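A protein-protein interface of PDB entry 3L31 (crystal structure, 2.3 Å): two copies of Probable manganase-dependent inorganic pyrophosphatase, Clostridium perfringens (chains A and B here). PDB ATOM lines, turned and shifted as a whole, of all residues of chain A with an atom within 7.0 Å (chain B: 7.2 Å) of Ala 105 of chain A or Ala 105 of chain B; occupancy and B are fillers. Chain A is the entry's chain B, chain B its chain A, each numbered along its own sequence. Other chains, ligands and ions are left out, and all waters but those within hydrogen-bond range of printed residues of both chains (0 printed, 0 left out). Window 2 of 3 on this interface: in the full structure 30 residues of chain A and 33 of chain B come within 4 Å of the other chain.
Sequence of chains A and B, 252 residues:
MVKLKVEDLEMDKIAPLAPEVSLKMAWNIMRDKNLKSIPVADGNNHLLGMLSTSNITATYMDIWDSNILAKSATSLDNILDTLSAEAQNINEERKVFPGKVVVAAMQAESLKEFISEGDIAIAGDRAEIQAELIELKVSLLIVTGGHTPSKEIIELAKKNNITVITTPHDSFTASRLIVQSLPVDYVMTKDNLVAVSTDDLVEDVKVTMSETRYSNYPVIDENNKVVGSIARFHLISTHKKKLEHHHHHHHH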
ATOM      1  N   VAL A 102     -21.243  -2.380  21.364  1.00  0.00           N
ATOM      2  CA  VAL A 102     -21.526  -3.620  20.660  1.00  0.00           C
ATOM      3  C   VAL A 102     -21.361  -3.411  19.111  1.00  0.00           C
ATOM      4  O   VAL A 102     -21.857  -2.423  18.537  1.00  0.00           O
ATOM      5  CB  VAL A 102     -22.952  -4.090  20.992  1.00  0.00           C
ATOM      6  CG1 VAL A 102     -23.229  -5.460  20.378  1.00  0.00           C
ATOM      7  CG2 VAL A 102     -23.158  -4.116  22.518  1.00  0.00           C
ATOM      8  N   VAL A 103     -20.579  -4.287  18.482  1.00  0.00           N
ATOM      9  CA  VAL A 103     -20.531  -4.397  17.025  1.00  0.00           C
ATOM     10  C   VAL A 103     -21.796  -5.122  16.548  1.00  0.00           C
ATOM     11  O   VAL A 103     -21.990  -6.285  16.815  1.00  0.00           O
ATOM     12  CB  VAL A 103     -19.251  -5.117  16.516  1.00  0.00           C
ATOM     13  CG1 VAL A 103     -19.324  -5.390  14.977  1.00  0.00           C
ATOM     14  CG2 VAL A 103     -18.024  -4.304  16.876  1.00  0.00           C
ATOM     15  N   ALA A 104     -22.663  -4.394  15.861  1.00  0.00           N
ATOM     16  CA  ALA A 104     -23.901  -4.950  15.342  1.00  0.00           C
ATOM     17  C   ALA A 104     -23.629  -5.868  14.167  1.00  0.00           C
ATOM     18  O   ALA A 104     -24.111  -5.633  13.086  1.00  0.00           O
ATOM     19  CB  ALA A 104     -24.856  -3.833  14.929  1.00  0.00           C
ATOM     20  N   ALA A 105     -22.848  -6.921  14.381  1.00  0.00           N
ATOM     21  CA  ALA A 105     -22.517  -7.892  13.296  1.00  0.00           C
ATOM     22  C   ALA A 105     -23.740  -8.750  12.910  1.00  0.00           C
ATOM     23  O   ALA A 105     -23.857  -9.277  11.806  1.00  0.00           O
ATOM     24  CB  ALA A 105     -21.279  -8.828  13.696  1.00  0.00           C
ATOM     25  N   MET A 106     -24.653  -8.844  13.857  1.00  0.00           N
ATOM     26  CA  MET A 106     -25.819  -9.713  13.759  1.00  0.00           C
ATOM     27  C   MET A 106     -26.787  -9.267  12.616  1.00  0.00           C
ATOM     28  O   MET A 106     -26.597  -8.220  11.981  1.00  0.00           O
ATOM     29  CB  MET A 106     -26.490  -9.785  15.157  1.00  0.00           C
ATOM     30  CG  MET A 106     -26.301  -8.495  15.996  1.00  0.00           C
ATOM     31  SD  MET A 106     -25.266  -8.521  17.515  1.00  0.00           S
ATOM     32  CE  MET A 106     -23.650  -9.133  17.015  1.00  0.00           C
ATOM     33  N   GLN A 107     -27.787 -10.098  12.324  1.00  0.00           N
ATOM     34  CA  GLN A 107     -28.868  -9.713  11.378  1.00  0.00           C
ATOM     35  C   GLN A 107     -30.040  -9.003  12.063  1.00  0.00           C
ATOM     36  O   GLN A 107     -30.216  -9.092  13.268  1.00  0.00           O
ATOM     37  CB  GLN A 107     -29.369 -10.924  10.595  1.00  0.00           C
ATOM     38  CG  GLN A 107     -28.303 -11.426   9.626  1.00  0.00           C
ATOM     39  CD  GLN A 107     -28.892 -12.025   8.360  1.00  0.00           C
ATOM     40  OE1 GLN A 107     -28.429 -11.744   7.239  1.00  0.00           O
ATOM     41  NE2 GLN A 107     -29.924 -12.855   8.530  1.00  0.00           N
ATOM     42  N   SER A 110     -32.355 -10.248  15.060  1.00  0.00           N
ATOM     43  CA  SER A 110     -31.562 -10.768  16.216  1.00  0.00           C
ATOM     44  C   SER A 110     -30.909  -9.687  17.119  1.00  0.00           C
ATOM     45  O   SER A 110     -30.493  -9.955  18.254  1.00  0.00           O
ATOM     46  CB  SER A 110     -30.490 -11.767  15.725  1.00  0.00           C
ATOM     47  OG  SER A 110     -29.532 -11.143  14.871  1.00  0.00           O
ATOM     48  N   LEU A 111     -30.826  -8.473  16.608  1.00  0.00           N
ATOM     49  CA  LEU A 111     -30.196  -7.365  17.340  1.00  0.00           C
ATOM     50  C   LEU A 111     -30.752  -7.198  18.759  1.00  0.00           C
ATOM     51  O   LEU A 111     -29.996  -6.948  19.706  1.00  0.00           O
ATOM     52  CB  LEU A 111     -30.341  -6.055  16.558  1.00  0.00           C
ATOM     53  CG  LEU A 111     -29.562  -5.940  15.234  1.00  0.00           C
ATOM     54  CD1 LEU A 111     -30.178  -4.920  14.311  1.00  0.00           C
ATOM     55  CD2 LEU A 111     -28.077  -5.604  15.471  1.00  0.00           C
ATOM     56  N   ILE A 115     -28.412  -6.033  21.827  1.00  0.00           N
ATOM     57  CA  ILE A 115     -28.363  -4.593  21.921  1.00  0.00           C
ATOM     58  C   ILE A 115     -29.561  -4.100  22.643  1.00  0.00           C
ATOM     59  O   ILE A 115     -30.685  -4.476  22.327  1.00  0.00           O
ATOM     60  CB  ILE A 115     -28.308  -3.940  20.539  1.00  0.00           C
ATOM     61  CG1 ILE A 115     -26.867  -3.875  20.068  1.00  0.00           C
ATOM     62  CG2 ILE A 115     -28.878  -2.546  20.588  1.00  0.00           C
ATOM     63  CD1 ILE A 115     -26.740  -3.934  18.605  1.00  0.00           C
ATOM     64  N   ILE A 122     -21.969   0.015  16.789  1.00  0.00           N
ATOM     65  CA  ILE A 122     -21.060   0.117  15.630  1.00  0.00           C
ATOM     66  C   ILE A 122     -21.639  -0.675  14.463  1.00  0.00           C
ATOM     67  O   ILE A 122     -21.762  -1.866  14.550  1.00  0.00           O
ATOM     68  CB  ILE A 122     -19.617  -0.385  15.950  1.00  0.00           C
ATOM     69  CG1 ILE A 122     -19.007   0.501  17.049  1.00  0.00           C
ATOM     70  CG2 ILE A 122     -18.732  -0.233  14.715  1.00  0.00           C
ATOM     71  CD1 ILE A 122     -17.583   0.126  17.572  1.00  0.00           C
ATOM     72  N   ALA A 123     -21.997  -0.002  13.380  1.00  0.00           N
ATOM     73  CA  ALA A 123     -22.773  -0.633  12.288  1.00  0.00           C
ATOM     74  C   ALA A 123     -22.159  -0.380  10.935  1.00  0.00           C
ATOM     75  O   ALA A 123     -21.403   0.535  10.785  1.00  0.00           O
ATOM     76  CB  ALA A 123     -24.225  -0.097  12.276  1.00  0.00           C
ATOM     77  N   GLY A 124     -22.545  -1.183   9.945  1.00  0.00           N
ATOM     78  CA  GLY A 124     -22.180  -0.933   8.534  1.00  0.00           C
ATOM     79  C   GLY A 124     -23.229  -0.166   7.724  1.00  0.00           C
ATOM     80  O   GLY A 124     -24.093   0.548   8.273  1.00  0.00           O
ATOM     81  N   ARG A 126     -25.963  -0.612   6.102  1.00  0.00           N
ATOM     82  CA  ARG A 126     -27.261  -1.219   5.849  1.00  0.00           C
ATOM     83  C   ARG A 126     -28.389  -0.426   6.476  1.00  0.00           C
ATOM     84  O   ARG A 126     -28.498  -0.342   7.693  1.00  0.00           O
ATOM     85  CB  ARG A 126     -27.260  -2.660   6.353  1.00  0.00           C
ATOM     86  CG  ARG A 126     -26.348  -3.586   5.538  1.00  0.00           C
ATOM     87  CD  ARG A 126     -26.553  -5.055   5.936  1.00  0.00           C
ATOM     88  NE  ARG A 126     -27.947  -5.482   5.741  1.00  0.00           N
ATOM     89  CZ  ARG A 126     -28.564  -6.395   6.500  1.00  0.00           C
ATOM     90  NH1 ARG A 126     -27.917  -6.962   7.521  1.00  0.00           N
ATOM     91  NH2 ARG A 126     -29.831  -6.723   6.257  1.00  0.00           N
ATOM     92  N   ILE A 129     -30.533  -2.169   9.157  1.00  0.00           N
ATOM     93  CA  ILE A 129     -29.848  -2.330  10.461  1.00  0.00           C
ATOM     94  C   ILE A 129     -29.800  -1.004  11.220  1.00  0.00           C
ATOM     95  O   ILE A 129     -30.062  -0.957  12.407  1.00  0.00           O
ATOM     96  CB  ILE A 129     -28.392  -2.882  10.318  1.00  0.00           C
ATOM     97  CG1 ILE A 129     -28.403  -4.253   9.658  1.00  0.00           C
ATOM     98  CG2 ILE A 129     -27.700  -2.993  11.649  1.00  0.00           C
ATOM     99  CD1 ILE A 129     -28.817  -5.372  10.590  1.00  0.00           C
ATOM    100  N   THR A 144     -19.621   2.944   9.908  1.00  0.00           N
ATOM    101  CA  THR A 144     -18.233   2.635   9.541  1.00  0.00           C
ATOM    102  C   THR A 144     -17.955   2.844   8.044  1.00  0.00           C
ATOM    103  O   THR A 144     -18.850   3.142   7.267  1.00  0.00           O
ATOM    104  CB  THR A 144     -17.925   1.167   9.840  1.00  0.00           C
ATOM    105  OG1 THR A 144     -18.775   0.365   9.029  1.00  0.00           O
ATOM    106  CG2 THR A 144     -18.211   0.855  11.236  1.00  0.00           C
ATOM    107  N   SER A 171     -15.135  -1.638  11.258  1.00  0.00           N
ATOM    108  CA  SER A 171     -15.531  -2.054  12.631  1.00  0.00           C
ATOM    109  C   SER A 171     -14.384  -2.509  13.536  1.00  0.00           C
ATOM    110  O   SER A 171     -14.365  -2.227  14.738  1.00  0.00           O
ATOM    111  CB  SER A 171     -16.471  -3.218  12.528  1.00  0.00           C
ATOM    112  OG  SER A 171     -17.596  -2.842  11.817  1.00  0.00           O
ATOM    113  N   VAL B 102     -10.540  -8.718  10.189  1.00  0.00           N
ATOM    114  CA  VAL B 102     -11.807  -8.151   9.800  1.00  0.00           C
ATOM    115  C   VAL B 102     -12.988  -8.764  10.635  1.00  0.00           C
ATOM    116  O   VAL B 102     -13.094  -9.992  10.807  1.00  0.00           O
ATOM    117  CB  VAL B 102     -11.997  -8.392   8.365  1.00  0.00           C
ATOM    118  CG1 VAL B 102     -13.265  -7.665   7.857  1.00  0.00           C
ATOM    119  CG2 VAL B 102     -10.750  -7.884   7.567  1.00  0.00           C
ATOM    120  N   VAL B 103     -13.851  -7.911  11.172  1.00  0.00           N
ATOM    121  CA  VAL B 103     -15.108  -8.374  11.773  1.00  0.00           C
ATOM    122  C   VAL B 103     -16.104  -8.679  10.653  1.00  0.00           C
ATOM    123  O   VAL B 103     -16.485  -7.794   9.926  1.00  0.00           O
ATOM    124  CB  VAL B 103     -15.717  -7.349  12.747  1.00  0.00           C
ATOM    125  CG1 VAL B 103     -17.058  -7.873  13.303  1.00  0.00           C
ATOM    126  CG2 VAL B 103     -14.708  -7.095  13.888  1.00  0.00           C
ATOM    127  N   ALA B 104     -16.447  -9.954  10.487  1.00  0.00           N
ATOM    128  CA  ALA B 104     -17.372 -10.363   9.453  1.00  0.00           C
ATOM    129  C   ALA B 104     -18.779  -9.858   9.783  1.00  0.00           C
ATOM    130  O   ALA B 104     -19.657 -10.602  10.140  1.00  0.00           O
ATOM    131  CB  ALA B 104     -17.351 -11.850   9.276  1.00  0.00           C
ATOM    132  N   ALA B 105     -18.973  -8.558   9.648  1.00  0.00           N
ATOM    133  CA  ALA B 105     -20.278  -7.890   9.970  1.00  0.00           C
ATOM    134  C   ALA B 105     -21.353  -8.203   8.938  1.00  0.00           C
ATOM    135  O   ALA B 105     -22.510  -8.459   9.273  1.00  0.00           O
ATOM    136  CB  ALA B 105     -20.123  -6.311  10.105  1.00  0.00           C
ATOM    137  N   MET B 106     -20.928  -8.194   7.687  1.00  0.00           N
ATOM    138  CA  MET B 106     -21.830  -8.382   6.537  1.00  0.00           C
ATOM    139  C   MET B 106     -22.553  -9.757   6.546  1.00  0.00           C
ATOM    140  O   MET B 106     -22.176 -10.659   7.298  1.00  0.00           O
ATOM    141  CB  MET B 106     -21.035  -8.149   5.218  1.00  0.00           C
ATOM    142  CG  MET B 106     -19.552  -8.620   5.216  1.00  0.00           C
ATOM    143  SD  MET B 106     -18.352  -7.655   6.206  1.00  0.00           S
ATOM    144  CE  MET B 106     -16.864  -8.658   6.127  1.00  0.00           C
ATOM    145  N   GLN B 107     -23.595  -9.878   5.720  1.00  0.00           N
ATOM    146  CA  GLN B 107     -24.237 -11.184   5.398  1.00  0.00           C
ATOM    147  C   GLN B 107     -23.418 -11.960   4.365  1.00  0.00           C
ATOM    148  O   GLN B 107     -22.541 -11.406   3.715  1.00  0.00           O
ATOM    149  CB  GLN B 107     -25.648 -11.014   4.822  1.00  0.00           C
ATOM    150  CG  GLN B 107     -26.312  -9.663   5.126  1.00  0.00           C
ATOM    151  CD  GLN B 107     -26.916  -9.041   3.871  1.00  0.00           C
ATOM    152  OE1 GLN B 107     -27.072  -9.724   2.852  1.00  0.00           O
ATOM    153  NE2 GLN B 107     -27.239  -7.744   3.930  1.00  0.00           N
ATOM    154  N   ALA B 108     -23.778 -13.225   4.167  1.00  0.00           N
ATOM    155  CA  ALA B 108     -22.890 -14.200   3.497  1.00  0.00           C
ATOM    156  C   ALA B 108     -22.364 -13.723   2.138  1.00  0.00           C
ATOM    157  O   ALA B 108     -21.157 -13.770   1.870  1.00  0.00           O
ATOM    158  CB  ALA B 108     -23.568 -15.593   3.369  1.00  0.00           C
ATOM    159  N   SER B 110     -21.933 -10.908   0.577  1.00  0.00           N
ATOM    160  CA  SER B 110     -21.063  -9.743   0.366  1.00  0.00           C
ATOM    161  C   SER B 110     -19.737  -9.783   1.144  1.00  0.00           C
ATOM    162  O   SER B 110     -18.992  -8.817   1.172  1.00  0.00           O
ATOM    163  CB  SER B 110     -21.832  -8.447   0.659  1.00  0.00           C
ATOM    164  OG  SER B 110     -21.972  -8.213   2.047  1.00  0.00           O
ATOM    165  N   LEU B 111     -19.452 -10.931   1.745  1.00  0.00           N
ATOM    166  CA  LEU B 111     -18.204 -11.145   2.492  1.00  0.00           C
ATOM    167  C   LEU B 111     -16.989 -11.020   1.568  1.00  0.00           C
ATOM    168  O   LEU B 111     -15.953 -10.485   1.957  1.00  0.00           O
ATOM    169  CB  LEU B 111     -18.201 -12.510   3.200  1.00  0.00           C
ATOM    170  CG  LEU B 111     -19.113 -12.684   4.435  1.00  0.00           C
ATOM    171  CD1 LEU B 111     -19.317 -14.129   4.773  1.00  0.00           C
ATOM    172  CD2 LEU B 111     -18.542 -11.965   5.675  1.00  0.00           C
ATOM    173  N   ILE B 115     -13.331  -9.534   2.603  1.00  0.00           N
ATOM    174  CA  ILE B 115     -12.474 -10.542   3.221  1.00  0.00           C
ATOM    175  C   ILE B 115     -11.741 -11.300   2.149  1.00  0.00           C
ATOM    176  O   ILE B 115     -12.340 -11.800   1.218  1.00  0.00           O
ATOM    177  CB  ILE B 115     -13.301 -11.505   4.107  1.00  0.00           C
ATOM    178  CG1 ILE B 115     -13.792 -10.730   5.317  1.00  0.00           C
ATOM    179  CG2 ILE B 115     -12.488 -12.713   4.525  1.00  0.00           C
ATOM    180  CD1 ILE B 115     -14.663 -11.489   6.219  1.00  0.00           C
ATOM    181  N   ILE B 122     -13.340 -12.523  12.305  1.00  0.00           N
ATOM    182  CA  ILE B 122     -14.040 -12.642  13.582  1.00  0.00           C
ATOM    183  C   ILE B 122     -15.527 -12.724  13.263  1.00  0.00           C
ATOM    184  O   ILE B 122     -16.121 -11.756  12.784  1.00  0.00           O
ATOM    185  CB  ILE B 122     -13.777 -11.380  14.445  1.00  0.00           C
ATOM    186  CG1 ILE B 122     -12.264 -11.201  14.602  1.00  0.00           C
ATOM    187  CG2 ILE B 122     -14.412 -11.490  15.804  1.00  0.00           C
ATOM    188  CD1 ILE B 122     -11.853 -10.077  15.575  1.00  0.00           C
ATOM    189  N   ALA B 123     -16.106 -13.894  13.469  1.00  0.00           N
ATOM    190  CA  ALA B 123     -17.492 -14.167  13.092  1.00  0.00           C
ATOM    191  C   ALA B 123     -18.304 -14.600  14.285  1.00  0.00           C
ATOM    192  O   ALA B 123     -17.738 -15.034  15.286  1.00  0.00           O
ATOM    193  CB  ALA B 123     -17.515 -15.280  12.105  1.00  0.00           C
ATOM    194  N   GLY B 124     -19.641 -14.538  14.145  1.00  0.00           N
ATOM    195  CA  GLY B 124     -20.572 -15.106  15.159  1.00  0.00           C
ATOM    196  C   GLY B 124     -21.022 -16.557  14.902  1.00  0.00           C
ATOM    197  O   GLY B 124     -20.390 -17.320  14.139  1.00  0.00           O
ATOM    198  N   ARG B 126     -23.153 -18.205  13.317  1.00  0.00           N
ATOM    199  CA  ARG B 126     -23.891 -18.601  12.122  1.00  0.00           C
ATOM    200  C   ARG B 126     -23.109 -19.506  11.158  1.00  0.00           C
ATOM    201  O   ARG B 126     -22.108 -19.107  10.558  1.00  0.00           O
ATOM    202  CB  ARG B 126     -24.363 -17.366  11.371  1.00  0.00           C
ATOM    203  CG  ARG B 126     -25.402 -16.530  12.087  1.00  0.00           C
ATOM    204  CD  ARG B 126     -25.888 -15.371  11.185  1.00  0.00           C
ATOM    205  NE  ARG B 126     -26.259 -15.819   9.821  1.00  0.00           N
ATOM    206  CZ  ARG B 126     -26.281 -15.031   8.738  1.00  0.00           C
ATOM    207  NH1 ARG B 126     -25.967 -13.735   8.829  1.00  0.00           N
ATOM    208  NH2 ARG B 126     -26.607 -15.533   7.554  1.00  0.00           N
ATOM    209  N   ILE B 129     -22.232 -18.136   7.642  1.00  0.00           N
ATOM    210  CA  ILE B 129     -21.111 -17.207   7.595  1.00  0.00           C
ATOM    211  C   ILE B 129     -19.761 -17.933   7.669  1.00  0.00           C
ATOM    212  O   ILE B 129     -18.851 -17.688   6.873  1.00  0.00           O
ATOM    213  CB  ILE B 129     -21.222 -16.121   8.655  1.00  0.00           C
ATOM    214  CG1 ILE B 129     -22.521 -15.341   8.446  1.00  0.00           C
ATOM    215  CG2 ILE B 129     -20.048 -15.142   8.561  1.00  0.00           C
ATOM    216  CD1 ILE B 129     -22.620 -14.689   7.103  1.00  0.00           C
ATOM    217  N   SER B 171     -17.398  -9.770  19.527  1.00  0.00           N
ATOM    218  CA  SER B 171     -16.487  -9.148  18.503  1.00  0.00           C
ATOM    219  C   SER B 171     -15.780  -7.864  18.969  1.00  0.00           C
ATOM    220  O   SER B 171     -14.643  -7.654  18.696  1.00  0.00           O
ATOM    221  CB  SER B 171     -17.237  -8.728  17.275  1.00  0.00           C
ATOM    222  OG  SER B 171     -18.132  -9.682  16.841  1.00  0.00           O
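O of Ala 105 of chain A sits close to O of Ala 105 of chain B (3.0 Å).
The side-chain amide nitrogen (NE2) of Gln 107 of chain B sits close to the guanidinium group (NE) of Arg 126 of chain A (3.0 Å).
The backbone carbonyl oxygen (O) of Gln 107 of chain A sits at hydrogen-bond distance from the side-chain hydroxyl (OG) of Ser 110 of chain A (2.7 Å).
Val 103 of chain A touches Val 103 of chain B (CG1 to CG1, 3.8 Å).
CG of Gln 107 of chain B touches OE1 of Gln 107 of chain A, at 3.6 Å.
NH1 of Arg 126 of chain B touches CG of Gln 107 of chain A (3.4 Å).
Of chain A, only Ala 105 comes within 4 Å of Ala 105 of chain B.
Of the printed residues of chain A, Gln 107 of chain B touches Gln 107 (3.6 Å) and Arg 126 (3.0 Å).
Of the printed residues of chain A, Val 103 of chain B touches Val 103 (3.8 Å).
Printed residues of chain A within 4 Å of Arg 126 of chain B: Gln 107.
Of the printed residues of chain B, Val 103 of chain A touches Val 103 (3.8 Å).
Printed residues of chain B within 4 Å of Arg 126 of chain A: Gln 107.
Ile 115 of chain B touches none of the printed residues of chain A.
The nearest residue of chain A that does not touch Ala 105 of chain B is Ser 171 of chain A (4.6 Å).
Hydrophobic or aromatic side chains of chain B that line the printed part of chain A: Val 103.
Printed residues of chain A that touch a printed residue of chain B: Val 103, Ala 105, Gln 107 and Arg 126.
Hydrophobic or aromatic side chains of chain A that line the printed part of chain B: Val 103 and Ala 105.
Among the printed residues, 5 pairs touch across the chains.
Among the printed residues, no Asp or Glu carboxylate lies within 4 Å of a Lys or Arg side-chain nitrogen of the other chain.
Val 103 of chain A touches its own counterpart, Val 103 of chain B.
Ala 105 of chain B touches its own counterpart, Ala 105 of chain A.
Gln 107 of chain B touches its own counterpart, Gln 107 of chain A.
Gln 107 of chain A touches Arg 126 of chain B, and with the chains exchanged Arg 126 of chain A touches Gln 107 of chain B.
15 positions are printed for both chains.
Of the 5 pairs that touch across the chains among the printed residues, 5 have their exchanged pair printed and touching as well.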
